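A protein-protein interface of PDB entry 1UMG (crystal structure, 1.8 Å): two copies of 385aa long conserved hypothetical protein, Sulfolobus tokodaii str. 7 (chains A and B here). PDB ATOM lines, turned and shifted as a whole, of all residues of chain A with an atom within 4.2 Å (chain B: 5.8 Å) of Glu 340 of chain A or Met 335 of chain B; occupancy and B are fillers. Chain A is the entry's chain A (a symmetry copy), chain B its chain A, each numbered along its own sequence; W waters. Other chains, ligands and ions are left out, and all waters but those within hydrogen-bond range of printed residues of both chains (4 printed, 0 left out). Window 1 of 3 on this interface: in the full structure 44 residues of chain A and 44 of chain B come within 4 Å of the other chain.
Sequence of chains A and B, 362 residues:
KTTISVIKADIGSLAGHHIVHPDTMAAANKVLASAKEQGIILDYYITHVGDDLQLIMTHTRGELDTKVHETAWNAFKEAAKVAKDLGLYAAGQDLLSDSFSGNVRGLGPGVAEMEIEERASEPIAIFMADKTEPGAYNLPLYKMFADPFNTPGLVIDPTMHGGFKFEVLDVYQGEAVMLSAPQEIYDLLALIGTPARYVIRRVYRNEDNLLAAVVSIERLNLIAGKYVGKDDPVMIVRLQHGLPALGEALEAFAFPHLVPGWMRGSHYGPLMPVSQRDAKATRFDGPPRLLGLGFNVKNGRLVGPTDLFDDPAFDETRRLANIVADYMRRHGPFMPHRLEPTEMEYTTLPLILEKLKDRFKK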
ATOM      1  N   GLY A 193      33.610   1.148 -17.438  1.00  0.00           N
ATOM      2  CA  GLY A 193      32.710   1.135 -16.296  1.00  0.00           C
ATOM      3  C   GLY A 193      31.291   0.892 -16.785  1.00  0.00           C
ATOM      4  O   GLY A 193      30.380   0.639 -15.994  1.00  0.00           O
ATOM      5  N   THR A 194      31.111   0.977 -18.101  1.00  0.00           N
ATOM      6  CA  THR A 194      29.821   0.749 -18.754  1.00  0.00           C
ATOM      7  C   THR A 194      29.998  -0.496 -19.631  1.00  0.00           C
ATOM      8  O   THR A 194      30.216  -0.393 -20.839  1.00  0.00           O
ATOM      9  CB  THR A 194      29.435   1.950 -19.653  1.00  0.00           C
ATOM     10  OG1 THR A 194      29.443   3.152 -18.872  1.00  0.00           O
ATOM     11  CG2 THR A 194      28.052   1.749 -20.261  1.00  0.00           C
ATOM     12  N   TYR A 268      21.002  -7.917 -12.560  1.00  0.00           N
ATOM     13  CA  TYR A 268      22.384  -7.823 -12.112  1.00  0.00           C
ATOM     14  C   TYR A 268      22.452  -8.834 -10.983  1.00  0.00           C
ATOM     15  O   TYR A 268      21.578  -8.861 -10.111  1.00  0.00           O
ATOM     16  CB  TYR A 268      22.718  -6.444 -11.544  1.00  0.00           C
ATOM     17  CG  TYR A 268      23.177  -5.454 -12.576  1.00  0.00           C
ATOM     18  CD1 TYR A 268      24.431  -5.570 -13.177  1.00  0.00           C
ATOM     19  CD2 TYR A 268      22.347  -4.413 -12.976  1.00  0.00           C
ATOM     20  CE1 TYR A 268      24.840  -4.670 -14.164  1.00  0.00           C
ATOM     21  CE2 TYR A 268      22.741  -3.515 -13.954  1.00  0.00           C
ATOM     22  CZ  TYR A 268      23.983  -3.646 -14.543  1.00  0.00           C
ATOM     23  OH  TYR A 268      24.347  -2.752 -15.525  1.00  0.00           O
ATOM     24  N   MET A 335      15.089  -1.749 -10.446  1.00  0.00           N
ATOM     25  CA  MET A 335      16.501  -1.477 -10.704  1.00  0.00           C
ATOM     26  C   MET A 335      17.016  -1.133  -9.302  1.00  0.00           C
ATOM     27  O   MET A 335      16.252  -0.636  -8.470  1.00  0.00           O
ATOM     28  CB  MET A 335      16.667  -0.262 -11.623  1.00  0.00           C
ATOM     29  CG  MET A 335      16.288  -0.501 -13.086  1.00  0.00           C
ATOM     30  SD  MET A 335      16.506   0.985 -14.099  1.00  0.00           S
ATOM     31  CE  MET A 335      18.310   1.115 -14.142  1.00  0.00           C
ATOM     32  N   ARG A 338      17.052  -5.259 -11.441  1.00  0.00           N
ATOM     33  CA  ARG A 338      16.576  -5.434 -12.815  1.00  0.00           C
ATOM     34  C   ARG A 338      17.460  -4.492 -13.646  1.00  0.00           C
ATOM     35  O   ARG A 338      17.846  -3.431 -13.162  1.00  0.00           O
ATOM     36  CB  ARG A 338      15.113  -5.003 -12.925  1.00  0.00           C
ATOM     37  CG  ARG A 338      14.410  -5.403 -14.220  1.00  0.00           C
ATOM     38  CD  ARG A 338      13.375  -4.346 -14.600  1.00  0.00           C
ATOM     39  NE  ARG A 338      14.036  -3.169 -15.154  1.00  0.00           N
ATOM     40  CZ  ARG A 338      13.461  -1.984 -15.335  1.00  0.00           C
ATOM     41  NH1 ARG A 338      14.165  -0.988 -15.855  1.00  0.00           N
ATOM     42  NH2 ARG A 338      12.197  -1.787 -14.985  1.00  0.00           N
ATOM     43  N   LEU A 339      17.781  -4.866 -14.881  1.00  0.00           N
ATOM     44  CA  LEU A 339      18.629  -4.021 -15.723  1.00  0.00           C
ATOM     45  C   LEU A 339      17.887  -2.789 -16.235  1.00  0.00           C
ATOM     46  O   LEU A 339      16.659  -2.727 -16.171  1.00  0.00           O
ATOM     47  CB  LEU A 339      19.153  -4.812 -16.929  1.00  0.00           C
ATOM     48  CG  LEU A 339      20.080  -6.003 -16.679  1.00  0.00           C
ATOM     49  CD1 LEU A 339      20.541  -6.584 -18.007  1.00  0.00           C
ATOM     50  CD2 LEU A 339      21.271  -5.562 -15.867  1.00  0.00           C
ATOM     51  N   GLU A 340      18.634  -1.811 -16.736  1.00  0.00           N
ATOM     52  CA  GLU A 340      18.008  -0.611 -17.281  1.00  0.00           C
ATOM     53  C   GLU A 340      17.129  -1.047 -18.455  1.00  0.00           C
ATOM     54  O   GLU A 340      17.396  -2.064 -19.094  1.00  0.00           O
ATOM     55  CB  GLU A 340      19.066   0.397 -17.734  1.00  0.00           C
ATOM     56  CG  GLU A 340      20.028  -0.110 -18.784  1.00  0.00           C
ATOM     57  CD  GLU A 340      21.204   0.830 -18.979  1.00  0.00           C
ATOM     58  OE1 GLU A 340      20.994   1.974 -19.442  1.00  0.00           O
ATOM     59  OE2 GLU A 340      22.341   0.425 -18.656  1.00  0.00           O
ATOM     60  N   PRO A 341      16.073  -0.279 -18.749  1.00  0.00           N
ATOM     61  CA  PRO A 341      15.119  -0.553 -19.832  1.00  0.00           C
ATOM     62  C   PRO A 341      15.660  -1.106 -21.150  1.00  0.00           C
ATOM     63  O   PRO A 341      15.217  -2.161 -21.614  1.00  0.00           O
ATOM     64  CB  PRO A 341      14.419   0.790 -20.018  1.00  0.00           C
ATOM     65  CG  PRO A 341      14.399   1.337 -18.632  1.00  0.00           C
ATOM     66  CD  PRO A 341      15.802   1.041 -18.149  1.00  0.00           C
ATOM     67  N   THR A 342      16.612  -0.404 -21.748  1.00  0.00           N
ATOM     68  CA  THR A 342      17.170  -0.812 -23.035  1.00  0.00           C
ATOM     69  C   THR A 342      18.094  -2.027 -23.014  1.00  0.00           C
ATOM     70  O   THR A 342      18.419  -2.576 -24.069  1.00  0.00           O
ATOM     71  CB  THR A 342      17.929   0.356 -23.695  1.00  0.00           C
ATOM     72  OG1 THR A 342      19.026   0.744 -22.861  1.00  0.00           O
ATOM     73  CG2 THR A 342      17.004   1.546 -23.885  1.00  0.00           C
ATOM     74  N   GLU A 343      18.512  -2.449 -21.824  1.00  0.00           N
ATOM     75  CA  GLU A 343      19.411  -3.594 -21.700  1.00  0.00           C
ATOM     76  C   GLU A 343      18.716  -4.911 -21.366  1.00  0.00           C
ATOM     77  O   GLU A 343      19.344  -5.969 -21.385  1.00  0.00           O
ATOM     78  CB  GLU A 343      20.476  -3.305 -20.644  1.00  0.00           C
ATOM     79  CG  GLU A 343      21.551  -2.350 -21.110  1.00  0.00           C
ATOM     80  CD  GLU A 343      22.308  -2.895 -22.300  1.00  0.00           C
ATOM     81  OE1 GLU A 343      22.848  -4.017 -22.191  1.00  0.00           O
ATOM     82  OE2 GLU A 343      22.364  -2.207 -23.339  1.00  0.00           O
ATOM     83  N   MET A 344      17.426  -4.845 -21.060  1.00  0.00           N
ATOM     84  CA  MET A 344      16.661  -6.038 -20.718  1.00  0.00           C
ATOM     85  C   MET A 344      16.441  -6.937 -21.934  1.00  0.00           C
ATOM     86  O   MET A 344      15.939  -6.484 -22.962  1.00  0.00           O
ATOM     87  CB  MET A 344      15.306  -5.632 -20.136  1.00  0.00           C
ATOM     88  CG  MET A 344      15.396  -4.840 -18.840  1.00  0.00           C
ATOM     89  SD  MET A 344      13.810  -4.087 -18.411  1.00  0.00           S
ATOM     90  CE  MET A 344      12.836  -5.555 -18.097  1.00  0.00           C
ATOM     91  N   HIS B 331      33.231  -2.241  -6.120  1.00  0.00           N
ATOM     92  CA  HIS B 331      33.039  -2.194  -7.572  1.00  0.00           C
ATOM     93  C   HIS B 331      33.706  -0.960  -8.174  1.00  0.00           C
ATOM     94  O   HIS B 331      33.844  -0.855  -9.393  1.00  0.00           O
ATOM     95  CB  HIS B 331      31.554  -2.143  -7.943  1.00  0.00           C
ATOM     96  CG  HIS B 331      30.816  -3.426  -7.718  1.00  0.00           C
ATOM     97  ND1 HIS B 331      30.427  -3.849  -6.469  1.00  0.00           N
ATOM     98  CD2 HIS B 331      30.383  -4.368  -8.589  1.00  0.00           C
ATOM     99  CE1 HIS B 331      29.779  -4.998  -6.579  1.00  0.00           C
ATOM    100  NE2 HIS B 331      29.741  -5.332  -7.855  1.00  0.00           N
ATOM    101  N   PRO B 333      34.386   2.465  -9.906  1.00  0.00           N
ATOM    102  CA  PRO B 333      33.608   3.191 -10.919  1.00  0.00           C
ATOM    103  C   PRO B 333      32.890   2.322 -11.951  1.00  0.00           C
ATOM    104  O   PRO B 333      32.642   2.765 -13.071  1.00  0.00           O
ATOM    105  CB  PRO B 333      34.660   4.092 -11.558  1.00  0.00           C
ATOM    106  CG  PRO B 333      35.855   3.183 -11.594  1.00  0.00           C
ATOM    107  CD  PRO B 333      35.828   2.527 -10.207  1.00  0.00           C
ATOM    108  N   PHE B 334      32.555   1.091 -11.578  1.00  0.00           N
ATOM    109  CA  PHE B 334      31.860   0.175 -12.483  1.00  0.00           C
ATOM    110  C   PHE B 334      30.374   0.037 -12.178  1.00  0.00           C
ATOM    111  O   PHE B 334      29.969   0.067 -11.017  1.00  0.00           O
ATOM    112  CB  PHE B 334      32.480  -1.225 -12.395  1.00  0.00           C
ATOM    113  CG  PHE B 334      33.814  -1.347 -13.072  1.00  0.00           C
ATOM    114  CD1 PHE B 334      33.898  -1.826 -14.376  1.00  0.00           C
ATOM    115  CD2 PHE B 334      34.982  -0.983 -12.411  1.00  0.00           C
ATOM    116  CE1 PHE B 334      35.132  -1.945 -15.013  1.00  0.00           C
ATOM    117  CE2 PHE B 334      36.220  -1.095 -13.036  1.00  0.00           C
ATOM    118  CZ  PHE B 334      36.294  -1.576 -14.344  1.00  0.00           C
ATOM    119  N   MET B 335      29.567  -0.111 -13.227  1.00  0.00           N
ATOM    120  CA  MET B 335      28.136  -0.343 -13.041  1.00  0.00           C
ATOM    121  C   MET B 335      28.118  -1.777 -12.498  1.00  0.00           C
ATOM    122  O   MET B 335      29.014  -2.564 -12.810  1.00  0.00           O
ATOM    123  CB  MET B 335      27.393  -0.293 -14.380  1.00  0.00           C
ATOM    124  CG  MET B 335      27.245   1.104 -14.985  1.00  0.00           C
ATOM    125  SD  MET B 335      26.363   1.071 -16.568  1.00  0.00           S
ATOM    126  CE  MET B 335      24.687   0.662 -16.025  1.00  0.00           C
ATOM    127  N   PRO B 336      27.094  -2.151 -11.716  1.00  0.00           N
ATOM    128  CA  PRO B 336      25.945  -1.353 -11.289  1.00  0.00           C
ATOM    129  C   PRO B 336      26.150  -0.440 -10.078  1.00  0.00           C
ATOM    130  O   PRO B 336      25.188   0.171  -9.614  1.00  0.00           O
ATOM    131  CB  PRO B 336      24.892  -2.414 -11.023  1.00  0.00           C
ATOM    132  CG  PRO B 336      25.709  -3.479 -10.373  1.00  0.00           C
ATOM    133  CD  PRO B 336      26.957  -3.540 -11.240  1.00  0.00           C
ATOM    134  N   HIS B 337      27.365  -0.357  -9.539  1.00  0.00           N
ATOM    135  CA  HIS B 337      27.573   0.544  -8.410  1.00  0.00           C
ATOM    136  C   HIS B 337      27.497   1.971  -8.961  1.00  0.00           C
ATOM    137  O   HIS B 337      26.856   2.841  -8.370  1.00  0.00           O
ATOM    138  CB  HIS B 337      28.922   0.299  -7.722  1.00  0.00           C
ATOM    139  CG  HIS B 337      29.228   1.276  -6.632  1.00  0.00           C
ATOM    140  ND1 HIS B 337      28.244   1.834  -5.832  1.00  0.00           N
ATOM    141  CD2 HIS B 337      30.397   1.802  -6.201  1.00  0.00           C
ATOM    142  CE1 HIS B 337      28.797   2.661  -4.965  1.00  0.00           C
ATOM    143  NE2 HIS B 337      30.108   2.660  -5.168  1.00  0.00           N
ATOM    144  N   ARG B 338      28.149   2.202 -10.097  1.00  0.00           N
ATOM    145  CA  ARG B 338      28.107   3.512 -10.750  1.00  0.00           C
ATOM    146  C   ARG B 338      26.804   3.491 -11.562  1.00  0.00           C
ATOM    147  O   ARG B 338      26.413   2.439 -12.063  1.00  0.00           O
ATOM    148  CB  ARG B 338      29.302   3.671 -11.691  1.00  0.00           C
ATOM    149  CG  ARG B 338      29.541   5.087 -12.210  1.00  0.00           C
ATOM    150  CD  ARG B 338      30.118   5.034 -13.623  1.00  0.00           C
ATOM    151  NE  ARG B 338      29.070   4.706 -14.584  1.00  0.00           N
ATOM    152  CZ  ARG B 338      29.278   4.325 -15.841  1.00  0.00           C
ATOM    153  NH1 ARG B 338      28.242   4.059 -16.624  1.00  0.00           N
ATOM    154  NH2 ARG B 338      30.512   4.197 -16.312  1.00  0.00           N
ATOM    155  N   LEU B 339      26.133   4.631 -11.695  1.00  0.00           N
ATOM    156  CA  LEU B 339      24.878   4.679 -12.447  1.00  0.00           C
ATOM    157  C   LEU B 339      25.104   4.578 -13.953  1.00  0.00           C
ATOM    158  O   LEU B 339      26.227   4.746 -14.429  1.00  0.00           O
ATOM    159  CB  LEU B 339      24.121   5.981 -12.153  1.00  0.00           C
ATOM    160  CG  LEU B 339      23.622   6.235 -10.729  1.00  0.00           C
ATOM    161  CD1 LEU B 339      22.833   7.534 -10.686  1.00  0.00           C
ATOM    162  CD2 LEU B 339      22.752   5.087 -10.281  1.00  0.00           C
ATOM    163  N   GLU B 340      24.039   4.296 -14.697  1.00  0.00           N
ATOM    164  CA  GLU B 340      24.155   4.215 -16.148  1.00  0.00           C
ATOM    165  C   GLU B 340      24.607   5.588 -16.648  1.00  0.00           C
ATOM    166  O   GLU B 340      24.339   6.606 -16.011  1.00  0.00           O
ATOM    167  CB  GLU B 340      22.821   3.814 -16.780  1.00  0.00           C
ATOM    168  CG  GLU B 340      21.666   4.744 -16.484  1.00  0.00           C
ATOM    169  CD  GLU B 340      20.334   4.145 -16.900  1.00  0.00           C
ATOM    170  OE1 GLU B 340      20.115   3.942 -18.116  1.00  0.00           O
ATOM    171  OE2 GLU B 340      19.508   3.868 -16.004  1.00  0.00           O
ATOM    172  N   PRO B 341      25.295   5.628 -17.796  1.00  0.00           N
ATOM    173  CA  PRO B 341      25.814   6.855 -18.415  1.00  0.00           C
ATOM    174  C   PRO B 341      24.951   8.115 -18.359  1.00  0.00           C
ATOM    175  O   PRO B 341      25.399   9.158 -17.875  1.00  0.00           O
ATOM    176  CB  PRO B 341      26.100   6.419 -19.849  1.00  0.00           C
ATOM    177  CG  PRO B 341      26.519   4.999 -19.677  1.00  0.00           C
ATOM    178  CD  PRO B 341      25.489   4.477 -18.699  1.00  0.00           C
HETATM  179  O   HOH W   1      18.092   2.695 -20.293  1.00  0.00           O
HETATM  180  O   HOH W   2      24.484   1.025 -19.760  1.00  0.00           O
HETATM  181  O   HOH W   3      22.277   4.842 -20.160  1.00  0.00           O
HETATM  182  O   HOH W   4      17.034   3.993 -16.195  1.00  0.00           O
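The guanidinium group (NH1) of Arg 338 of chain B sits close to the side-chain sulfur (SD) of Met 335 of chain B.
The side-chain sulfur (SD) of Met 335 of chain A lies close to the guanidinium group (NH1) of Arg 338 of chain A (3.5 Å).
Printed residues of chain A that touch a printed residue of chain B: Gly 193, Thr 194, Tyr 268, Met 335 and Glu 340.
Printed residues of chain B that touch a printed residue of chain A: Pro 333, Phe 334, Met 335, Pro 336, Arg 338, Glu 340 and Pro 341.
Hydrophobic or aromatic side chains of chain B within 4 Å of the printed part of chain A: Phe 334, Met 335, Pro 336 and Pro 341.
Along chain B the printed residues that touch a printed residue of chain A span positions 333 to 341.
Among the printed residues, no Asp or Glu carboxylate lies within 4 Å of a Lys or Arg side-chain nitrogen of the other chain.
N of Met 335 of chain B sits at hydrogen-bond distance from O of Gly 193 of chain A, 3.0 Å away.
NH1 of Arg 338 of chain B lies within hydrogen-bond range of OG1 of Thr 194 of chain A (2.7 Å).
The side-chain carboxylate (OE1) of Glu 340 of chain B lies close to the side-chain carboxylate (OE1) of Glu 340 of chain A (2.5 Å).
Met 335 of chain A touches Glu 340 of chain B, and with the chains exchanged Glu 340 of chain A touches Met 335 of chain B.
Glu 340 of chain A touches its own counterpart, Glu 340 of chain B.
Of the 11 pairs that touch across the chains among the printed residues, 3 have their exchanged pair printed and touching as well.
Water W4 lies within hydrogen-bond range of OE2 of Glu 340 of chain B and SD of Met 335 of chain A.
Water W2 lies within hydrogen-bond range of OE2 of Glu 340 of chain A (2.5 Å) and SD of Met 335 of chain B (3.7 Å).
Water W3 bridges the side-chain carboxylate (OE1) of Glu 340 of chain B and the side-chain carboxylate (OE1) of Glu 340 of chain A.
Water W1 lies within hydrogen-bond range of the side-chain carboxylate of Glu 340 of chain A, the side-chain carboxylate of Glu 340 of chain B and the side-chain hydroxyl of Thr 342 of chain A.
Of chain B, only Met 335 and Glu 340 come within 4 Å of Glu 340 of chain A.
Printed residues of chain A within 4 Å of Met 335 of chain B: Gly 193, Tyr 268 and Glu 340.
Printed residues of chain B within 4 Å of Met 335 of chain A: Glu 340.
Of the printed residues of chain A, Phe 334 of chain B touches Gly 193.
Of the printed residues of chain B, Thr 194 of chain A touches Arg 338 and Pro 341.
Of the printed residues of chain A, Arg 338 of chain B touches Gly 193 (3.4 Å) and Thr 194 (2.7 Å).
The nearest residue of chain A that does not touch Met 335 of chain B is Thr 194 of chain A (4.1 Å).
Among the printed residues, pairs that only touch across the chains: Gly 193 of chain A with Arg 338 of chain B (3.4 Å), Tyr 268 of chain A with Met 335 of chain B (3.5 Å), Met 335 of chain A with Glu 340 of chain B (3.5 Å), Glu 340 of chain A with Met 335 of chain B (3.5 Å), Thr 194 of chain A with Pro 341 of chain B (3.6 Å), Gly 193 of chain A with Pro 333 of chain B (3.6 Å), Gly 193 of chain A with Phe 334 of chain B (3.7 Å) and Tyr 268 of chain A with Pro 336 of chain B (3.7 Å).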
